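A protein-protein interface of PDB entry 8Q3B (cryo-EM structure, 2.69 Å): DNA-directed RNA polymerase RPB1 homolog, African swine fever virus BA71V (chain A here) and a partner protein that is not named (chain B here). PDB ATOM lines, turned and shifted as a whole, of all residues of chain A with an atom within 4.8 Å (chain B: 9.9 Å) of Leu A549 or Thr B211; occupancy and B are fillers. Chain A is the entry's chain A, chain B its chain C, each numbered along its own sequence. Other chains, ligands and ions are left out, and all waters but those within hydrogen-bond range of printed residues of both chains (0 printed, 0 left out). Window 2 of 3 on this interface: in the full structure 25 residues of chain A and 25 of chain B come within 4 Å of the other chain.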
ATOM      1  N   VAL A 521      -1.126 -22.654 -14.361  1.00  0.00           N
ATOM      2  CA  VAL A 521      -1.300 -21.953 -13.098  1.00  0.00           C
ATOM      3  C   VAL A 521      -2.730 -22.146 -12.613  1.00  0.00           C
ATOM      4  O   VAL A 521      -3.646 -22.422 -13.389  1.00  0.00           O
ATOM      5  CB  VAL A 521      -0.978 -20.449 -13.218  1.00  0.00           C
ATOM      6  CG1 VAL A 521       0.522 -20.227 -13.224  1.00  0.00           C
ATOM      7  CG2 VAL A 521      -1.614 -19.864 -14.468  1.00  0.00           C
ATOM      8  N   MET A 522      -2.907 -21.997 -11.302  1.00  0.00           N
ATOM      9  CA  MET A 522      -4.215 -22.073 -10.674  1.00  0.00           C
ATOM     10  C   MET A 522      -4.307 -20.995  -9.606  1.00  0.00           C
ATOM     11  O   MET A 522      -3.294 -20.572  -9.046  1.00  0.00           O
ATOM     12  CB  MET A 522      -4.471 -23.450 -10.045  1.00  0.00           C
ATOM     13  CG  MET A 522      -3.342 -23.955  -9.161  1.00  0.00           C
ATOM     14  SD  MET A 522      -3.423 -25.730  -8.861  1.00  0.00           S
ATOM     15  CE  MET A 522      -2.371 -26.339 -10.174  1.00  0.00           C
ATOM     16  N   ASN A 523      -5.530 -20.555  -9.327  1.00  0.00           N
ATOM     17  CA  ASN A 523      -5.742 -19.543  -8.305  1.00  0.00           C
ATOM     18  C   ASN A 523      -5.614 -20.173  -6.918  1.00  0.00           C
ATOM     19  O   ASN A 523      -5.339 -21.366  -6.770  1.00  0.00           O
ATOM     20  CB  ASN A 523      -7.102 -18.874  -8.486  1.00  0.00           C
ATOM     21  CG  ASN A 523      -8.242 -19.869  -8.539  1.00  0.00           C
ATOM     22  OD1 ASN A 523      -8.046 -21.067  -8.344  1.00  0.00           O
ATOM     23  ND2 ASN A 523      -9.444 -19.375  -8.803  1.00  0.00           N
ATOM     24  N   THR A 547      -6.498 -13.652  -5.844  1.00  0.00           N
ATOM     25  CA  THR A 547      -6.168 -13.490  -7.253  1.00  0.00           C
ATOM     26  C   THR A 547      -4.778 -14.009  -7.602  1.00  0.00           C
ATOM     27  O   THR A 547      -4.405 -13.987  -8.779  1.00  0.00           O
ATOM     28  CB  THR A 547      -6.270 -12.015  -7.656  1.00  0.00           C
ATOM     29  OG1 THR A 547      -5.135 -11.300  -7.153  1.00  0.00           O
ATOM     30  CG2 THR A 547      -7.547 -11.393  -7.109  1.00  0.00           C
ATOM     31  N   ASP A 548      -4.008 -14.470  -6.620  1.00  0.00           N
ATOM     32  CA  ASP A 548      -2.672 -14.974  -6.895  1.00  0.00           C
ATOM     33  C   ASP A 548      -2.743 -16.258  -7.715  1.00  0.00           C
ATOM     34  O   ASP A 548      -3.728 -16.999  -7.677  1.00  0.00           O
ATOM     35  CB  ASP A 548      -1.915 -15.226  -5.592  1.00  0.00           C
ATOM     36  CG  ASP A 548      -1.375 -13.952  -4.976  1.00  0.00           C
ATOM     37  OD1 ASP A 548      -1.730 -12.857  -5.461  1.00  0.00           O
ATOM     38  OD2 ASP A 548      -0.593 -14.043  -4.005  1.00  0.00           O
ATOM     39  N   LEU A 549      -1.675 -16.515  -8.466  1.00  0.00           N
ATOM     40  CA  LEU A 549      -1.579 -17.676  -9.339  1.00  0.00           C
ATOM     41  C   LEU A 549      -0.479 -18.596  -8.835  1.00  0.00           C
ATOM     42  O   LEU A 549       0.627 -18.138  -8.527  1.00  0.00           O
ATOM     43  CB  LEU A 549      -1.298 -17.256 -10.783  1.00  0.00           C
ATOM     44  CG  LEU A 549      -2.386 -16.421 -11.461  1.00  0.00           C
ATOM     45  CD1 LEU A 549      -1.904 -15.915 -12.808  1.00  0.00           C
ATOM     46  CD2 LEU A 549      -3.666 -17.226 -11.619  1.00  0.00           C
ATOM     47  N   LEU A 550      -0.784 -19.888  -8.754  1.00  0.00           N
ATOM     48  CA  LEU A 550       0.150 -20.899  -8.282  1.00  0.00           C
ATOM     49  C   LEU A 550       0.355 -21.947  -9.365  1.00  0.00           C
ATOM     50  O   LEU A 550      -0.604 -22.383 -10.007  1.00  0.00           O
ATOM     51  CB  LEU A 550      -0.364 -21.574  -7.008  1.00  0.00           C
ATOM     52  CG  LEU A 550      -0.324 -20.740  -5.729  1.00  0.00           C
ATOM     53  CD1 LEU A 550      -1.594 -19.923  -5.581  1.00  0.00           C
ATOM     54  CD2 LEU A 550      -0.125 -21.638  -4.523  1.00  0.00           C
ATOM     55  N   ASP A 551       1.606 -22.346  -9.568  1.00  0.00           N
ATOM     56  CA  ASP A 551       1.903 -23.422 -10.496  1.00  0.00           C
ATOM     57  C   ASP A 551       1.702 -24.774  -9.821  1.00  0.00           C
ATOM     58  O   ASP A 551       1.688 -24.889  -8.592  1.00  0.00           O
ATOM     59  CB  ASP A 551       3.337 -23.310 -11.013  1.00  0.00           C
ATOM     60  CG  ASP A 551       3.745 -21.881 -11.299  1.00  0.00           C
ATOM     61  OD1 ASP A 551       4.072 -21.151 -10.341  1.00  0.00           O
ATOM     62  OD2 ASP A 551       3.743 -21.488 -12.485  1.00  0.00           O
ATOM     63  N   ARG B  52     -20.666 -19.471  -8.839  1.00  0.00           N
ATOM     64  CA  ARG B  52     -20.997 -20.714  -9.525  1.00  0.00           C
ATOM     65  C   ARG B  52     -21.424 -21.796  -8.543  1.00  0.00           C
ATOM     66  O   ARG B  52     -22.277 -22.630  -8.871  1.00  0.00           O
ATOM     67  CB  ARG B  52     -19.795 -21.184 -10.345  1.00  0.00           C
ATOM     68  CG  ARG B  52     -19.820 -22.654 -10.742  1.00  0.00           C
ATOM     69  CD  ARG B  52     -18.605 -23.012 -11.580  1.00  0.00           C
ATOM     70  NE  ARG B  52     -17.362 -22.610 -10.933  1.00  0.00           N
ATOM     71  CZ  ARG B  52     -16.202 -22.460 -11.557  1.00  0.00           C
ATOM     72  NH1 ARG B  52     -16.081 -22.672 -12.857  1.00  0.00           N
ATOM     73  NH2 ARG B  52     -15.134 -22.087 -10.858  1.00  0.00           N
ATOM     74  N   ILE B 189     -17.488 -15.638 -19.492  1.00  0.00           N
ATOM     75  CA  ILE B 189     -16.267 -16.112 -20.130  1.00  0.00           C
ATOM     76  C   ILE B 189     -16.489 -16.181 -21.635  1.00  0.00           C
ATOM     77  O   ILE B 189     -17.494 -16.734 -22.098  1.00  0.00           O
ATOM     78  CB  ILE B 189     -15.848 -17.486 -19.577  1.00  0.00           C
ATOM     79  CG1 ILE B 189     -15.837 -17.471 -18.047  1.00  0.00           C
ATOM     80  CG2 ILE B 189     -14.478 -17.875 -20.106  1.00  0.00           C
ATOM     81  CD1 ILE B 189     -15.731 -18.842 -17.429  1.00  0.00           C
ATOM     82  N   TYR B 205     -13.788 -22.592 -23.760  1.00  0.00           N
ATOM     83  CA  TYR B 205     -13.719 -21.364 -22.982  1.00  0.00           C
ATOM     84  C   TYR B 205     -12.319 -20.775 -23.077  1.00  0.00           C
ATOM     85  O   TYR B 205     -11.329 -21.506 -23.142  1.00  0.00           O
ATOM     86  CB  TYR B 205     -14.073 -21.628 -21.519  1.00  0.00           C
ATOM     87  CG  TYR B 205     -15.557 -21.702 -21.241  1.00  0.00           C
ATOM     88  CD1 TYR B 205     -16.378 -20.603 -21.443  1.00  0.00           C
ATOM     89  CD2 TYR B 205     -16.135 -22.868 -20.765  1.00  0.00           C
ATOM     90  CE1 TYR B 205     -17.732 -20.668 -21.188  1.00  0.00           C
ATOM     91  CE2 TYR B 205     -17.486 -22.940 -20.505  1.00  0.00           C
ATOM     92  CZ  TYR B 205     -18.280 -21.839 -20.718  1.00  0.00           C
ATOM     93  OH  TYR B 205     -19.628 -21.910 -20.461  1.00  0.00           O
ATOM     94  N   LYS B 206     -12.243 -19.445 -23.085  1.00  0.00           N
ATOM     95  CA  LYS B 206     -10.959 -18.766 -23.205  1.00  0.00           C
ATOM     96  C   LYS B 206     -10.186 -18.711 -21.894  1.00  0.00           C
ATOM     97  O   LYS B 206      -9.029 -18.277 -21.900  1.00  0.00           O
ATOM     98  CB  LYS B 206     -11.165 -17.345 -23.733  1.00  0.00           C
ATOM     99  CG  LYS B 206     -11.406 -17.272 -25.231  1.00  0.00           C
ATOM    100  CD  LYS B 206     -11.210 -15.860 -25.757  1.00  0.00           C
ATOM    101  CE  LYS B 206     -11.333 -15.806 -27.270  1.00  0.00           C
ATOM    102  NZ  LYS B 206     -12.725 -16.058 -27.729  1.00  0.00           N
ATOM    103  N   GLN B 207     -10.783 -19.132 -20.783  1.00  0.00           N
ATOM    104  CA  GLN B 207     -10.130 -19.127 -19.482  1.00  0.00           C
ATOM    105  C   GLN B 207     -10.143 -20.529 -18.893  1.00  0.00           C
ATOM    106  O   GLN B 207     -11.153 -21.234 -18.963  1.00  0.00           O
ATOM    107  CB  GLN B 207     -10.820 -18.160 -18.518  1.00  0.00           C
ATOM    108  CG  GLN B 207     -10.899 -16.733 -19.021  1.00  0.00           C
ATOM    109  CD  GLN B 207     -11.345 -15.767 -17.945  1.00  0.00           C
ATOM    110  OE1 GLN B 207     -11.117 -15.995 -16.757  1.00  0.00           O
ATOM    111  NE2 GLN B 207     -11.985 -14.678 -18.354  1.00  0.00           N
ATOM    112  N   SER B 208      -9.016 -20.927 -18.310  1.00  0.00           N
ATOM    113  CA  SER B 208      -8.935 -22.219 -17.647  1.00  0.00           C
ATOM    114  C   SER B 208      -9.815 -22.234 -16.403  1.00  0.00           C
ATOM    115  O   SER B 208      -9.959 -21.228 -15.702  1.00  0.00           O
ATOM    116  CB  SER B 208      -7.490 -22.533 -17.268  1.00  0.00           C
ATOM    117  OG  SER B 208      -7.381 -23.835 -16.722  1.00  0.00           O
ATOM    118  N   SER B 209     -10.411 -23.395 -16.130  1.00  0.00           N
ATOM    119  CA  SER B 209     -11.273 -23.528 -14.962  1.00  0.00           C
ATOM    120  C   SER B 209     -10.508 -23.358 -13.658  1.00  0.00           C
ATOM    121  O   SER B 209     -11.122 -23.060 -12.628  1.00  0.00           O
ATOM    122  CB  SER B 209     -11.971 -24.886 -14.973  1.00  0.00           C
ATOM    123  OG  SER B 209     -11.056 -25.925 -15.267  1.00  0.00           O
ATOM    124  N   MET B 210      -9.188 -23.541 -13.676  1.00  0.00           N
ATOM    125  CA  MET B 210      -8.383 -23.413 -12.469  1.00  0.00           C
ATOM    126  C   MET B 210      -8.107 -21.964 -12.095  1.00  0.00           C
ATOM    127  O   MET B 210      -7.650 -21.709 -10.976  1.00  0.00           O
ATOM    128  CB  MET B 210      -7.060 -24.158 -12.648  1.00  0.00           C
ATOM    129  CG  MET B 210      -7.217 -25.551 -13.230  1.00  0.00           C
ATOM    130  SD  MET B 210      -6.124 -26.768 -12.478  1.00  0.00           S
ATOM    131  CE  MET B 210      -6.745 -26.809 -10.799  1.00  0.00           C
ATOM    132  N   THR B 211      -8.366 -21.017 -12.997  1.00  0.00           N
ATOM    133  CA  THR B 211      -8.216 -19.599 -12.710  1.00  0.00           C
ATOM    134  C   THR B 211      -9.492 -18.801 -12.917  1.00  0.00           C
ATOM    135  O   THR B 211      -9.592 -17.688 -12.388  1.00  0.00           O
ATOM    136  CB  THR B 211      -7.115 -18.983 -13.588  1.00  0.00           C
ATOM    137  OG1 THR B 211      -7.558 -18.931 -14.949  1.00  0.00           O
ATOM    138  CG2 THR B 211      -5.837 -19.801 -13.506  1.00  0.00           C
ATOM    139  N   SER B 212     -10.460 -19.327 -13.662  1.00  0.00           N
ATOM    140  CA  SER B 212     -11.679 -18.587 -13.948  1.00  0.00           C
ATOM    141  C   SER B 212     -12.594 -18.555 -12.731  1.00  0.00           C
ATOM    142  O   SER B 212     -12.697 -19.532 -11.983  1.00  0.00           O
ATOM    143  CB  SER B 212     -12.404 -19.219 -15.134  1.00  0.00           C
ATOM    144  OG  SER B 212     -13.806 -19.081 -15.006  1.00  0.00           O
ATOM    145  N   ASP B 213     -13.258 -17.418 -12.533  1.00  0.00           N
ATOM    146  CA  ASP B 213     -14.222 -17.225 -11.449  1.00  0.00           C
ATOM    147  C   ASP B 213     -15.474 -16.590 -12.039  1.00  0.00           C
ATOM    148  O   ASP B 213     -15.699 -15.380 -11.895  1.00  0.00           O
ATOM    149  CB  ASP B 213     -13.634 -16.363 -10.332  1.00  0.00           C
ATOM    150  CG  ASP B 213     -14.673 -15.941  -9.313  1.00  0.00           C
ATOM    151  OD1 ASP B 213     -15.506 -16.787  -8.927  1.00  0.00           O
ATOM    152  OD2 ASP B 213     -14.657 -14.763  -8.899  1.00  0.00           O
ATOM    153  N   PRO B 214     -16.309 -17.371 -12.720  1.00  0.00           N
ATOM    154  CA  PRO B 214     -17.485 -16.792 -13.375  1.00  0.00           C
ATOM    155  C   PRO B 214     -18.517 -16.310 -12.370  1.00  0.00           C
ATOM    156  O   PRO B 214     -18.614 -16.813 -11.249  1.00  0.00           O
ATOM    157  CB  PRO B 214     -18.026 -17.952 -14.216  1.00  0.00           C
ATOM    158  CG  PRO B 214     -17.589 -19.170 -13.492  1.00  0.00           C
ATOM    159  CD  PRO B 214     -16.278 -18.840 -12.837  1.00  0.00           C
ATOM    160  N   TYR B 299     -14.551 -18.831   1.840  1.00  0.00           N
ATOM    161  CA  TYR B 299     -13.394 -18.324   1.114  1.00  0.00           C
ATOM    162  C   TYR B 299     -13.612 -16.882   0.676  1.00  0.00           C
ATOM    163  O   TYR B 299     -12.700 -16.053   0.767  1.00  0.00           O
ATOM    164  CB  TYR B 299     -13.114 -19.220  -0.091  1.00  0.00           C
ATOM    165  CG  TYR B 299     -12.100 -18.664  -1.060  1.00  0.00           C
ATOM    166  CD1 TYR B 299     -10.765 -18.544  -0.705  1.00  0.00           C
ATOM    167  CD2 TYR B 299     -12.477 -18.272  -2.335  1.00  0.00           C
ATOM    168  CE1 TYR B 299      -9.837 -18.042  -1.592  1.00  0.00           C
ATOM    169  CE2 TYR B 299     -11.555 -17.769  -3.228  1.00  0.00           C
ATOM    170  CZ  TYR B 299     -10.237 -17.657  -2.852  1.00  0.00           C
ATOM    171  OH  TYR B 299      -9.316 -17.157  -3.741  1.00  0.00           O
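The side-chain amide oxygen (OD1) of Asn A523 lies close to the backbone carbonyl oxygen (O) of Met B210 (2.7 Å).
N of Leu A550 is in hydrogen-bond range of O of Met A522 (2.6 Å).
The backbone carbonyl oxygen (O) of Ser B208 is in hydrogen-bond range of the side-chain hydroxyl (OG1) of Thr B211 (3.4 Å).
Among the printed residues, merely in contact across the chains: Val A521 with Thr B211, Met A522 with Met B210, Leu A549 with Thr B211, Val A521 with Met B210, Asn A523 with Thr B211 and Met A522 with Thr B211.
Leu A549 touches just one residue of chain B: Thr B211 (3.9 Å).
Of chain A, only Val A521 (3.4 Å), Met A522 (3.98 Å), Asn A523 (3.96 Å) and Leu A549 (3.9 Å) come within 4 Å of Thr B211.
No residue of chain B comes within 4 Å of Leu A550.
Of the printed residues of chain B, Asn A523 touches Met B210 and Thr B211.
Printed residues of chain A within 4 Å of Met B210: Val A521 (3.9 Å), Met A522 (3.5 Å) and Asn A523 (2.7 Å).
Printed residues of chain B within 4 Å of Met A522: Met B210 (3.5 Å) and Thr B211 (3.98 Å).
Ser B212 touches none of the printed residues of chain A.
The nearest residue of chain B that does not touch Leu A549 is Met B210 (6.0 Å).
The nearest printed residue of chain A that does not touch Thr B211 is Asp A548 (6.8 Å).
The nearest printed residue of chain A that does not touch Met B210 is Leu A549 (6.0 Å).
Hydrophobic or aromatic side chains of chain B that line the printed part of chain A: Met B210.
Along chain B the printed residues that touch a printed residue of chain A span positions 210 to 211.
Among the printed residues, 7 pairs touch across the chains.
Among the printed residues, no Asp or Glu carboxylate lies within 4 Å of a Lys or Arg side-chain nitrogen of the other chain.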
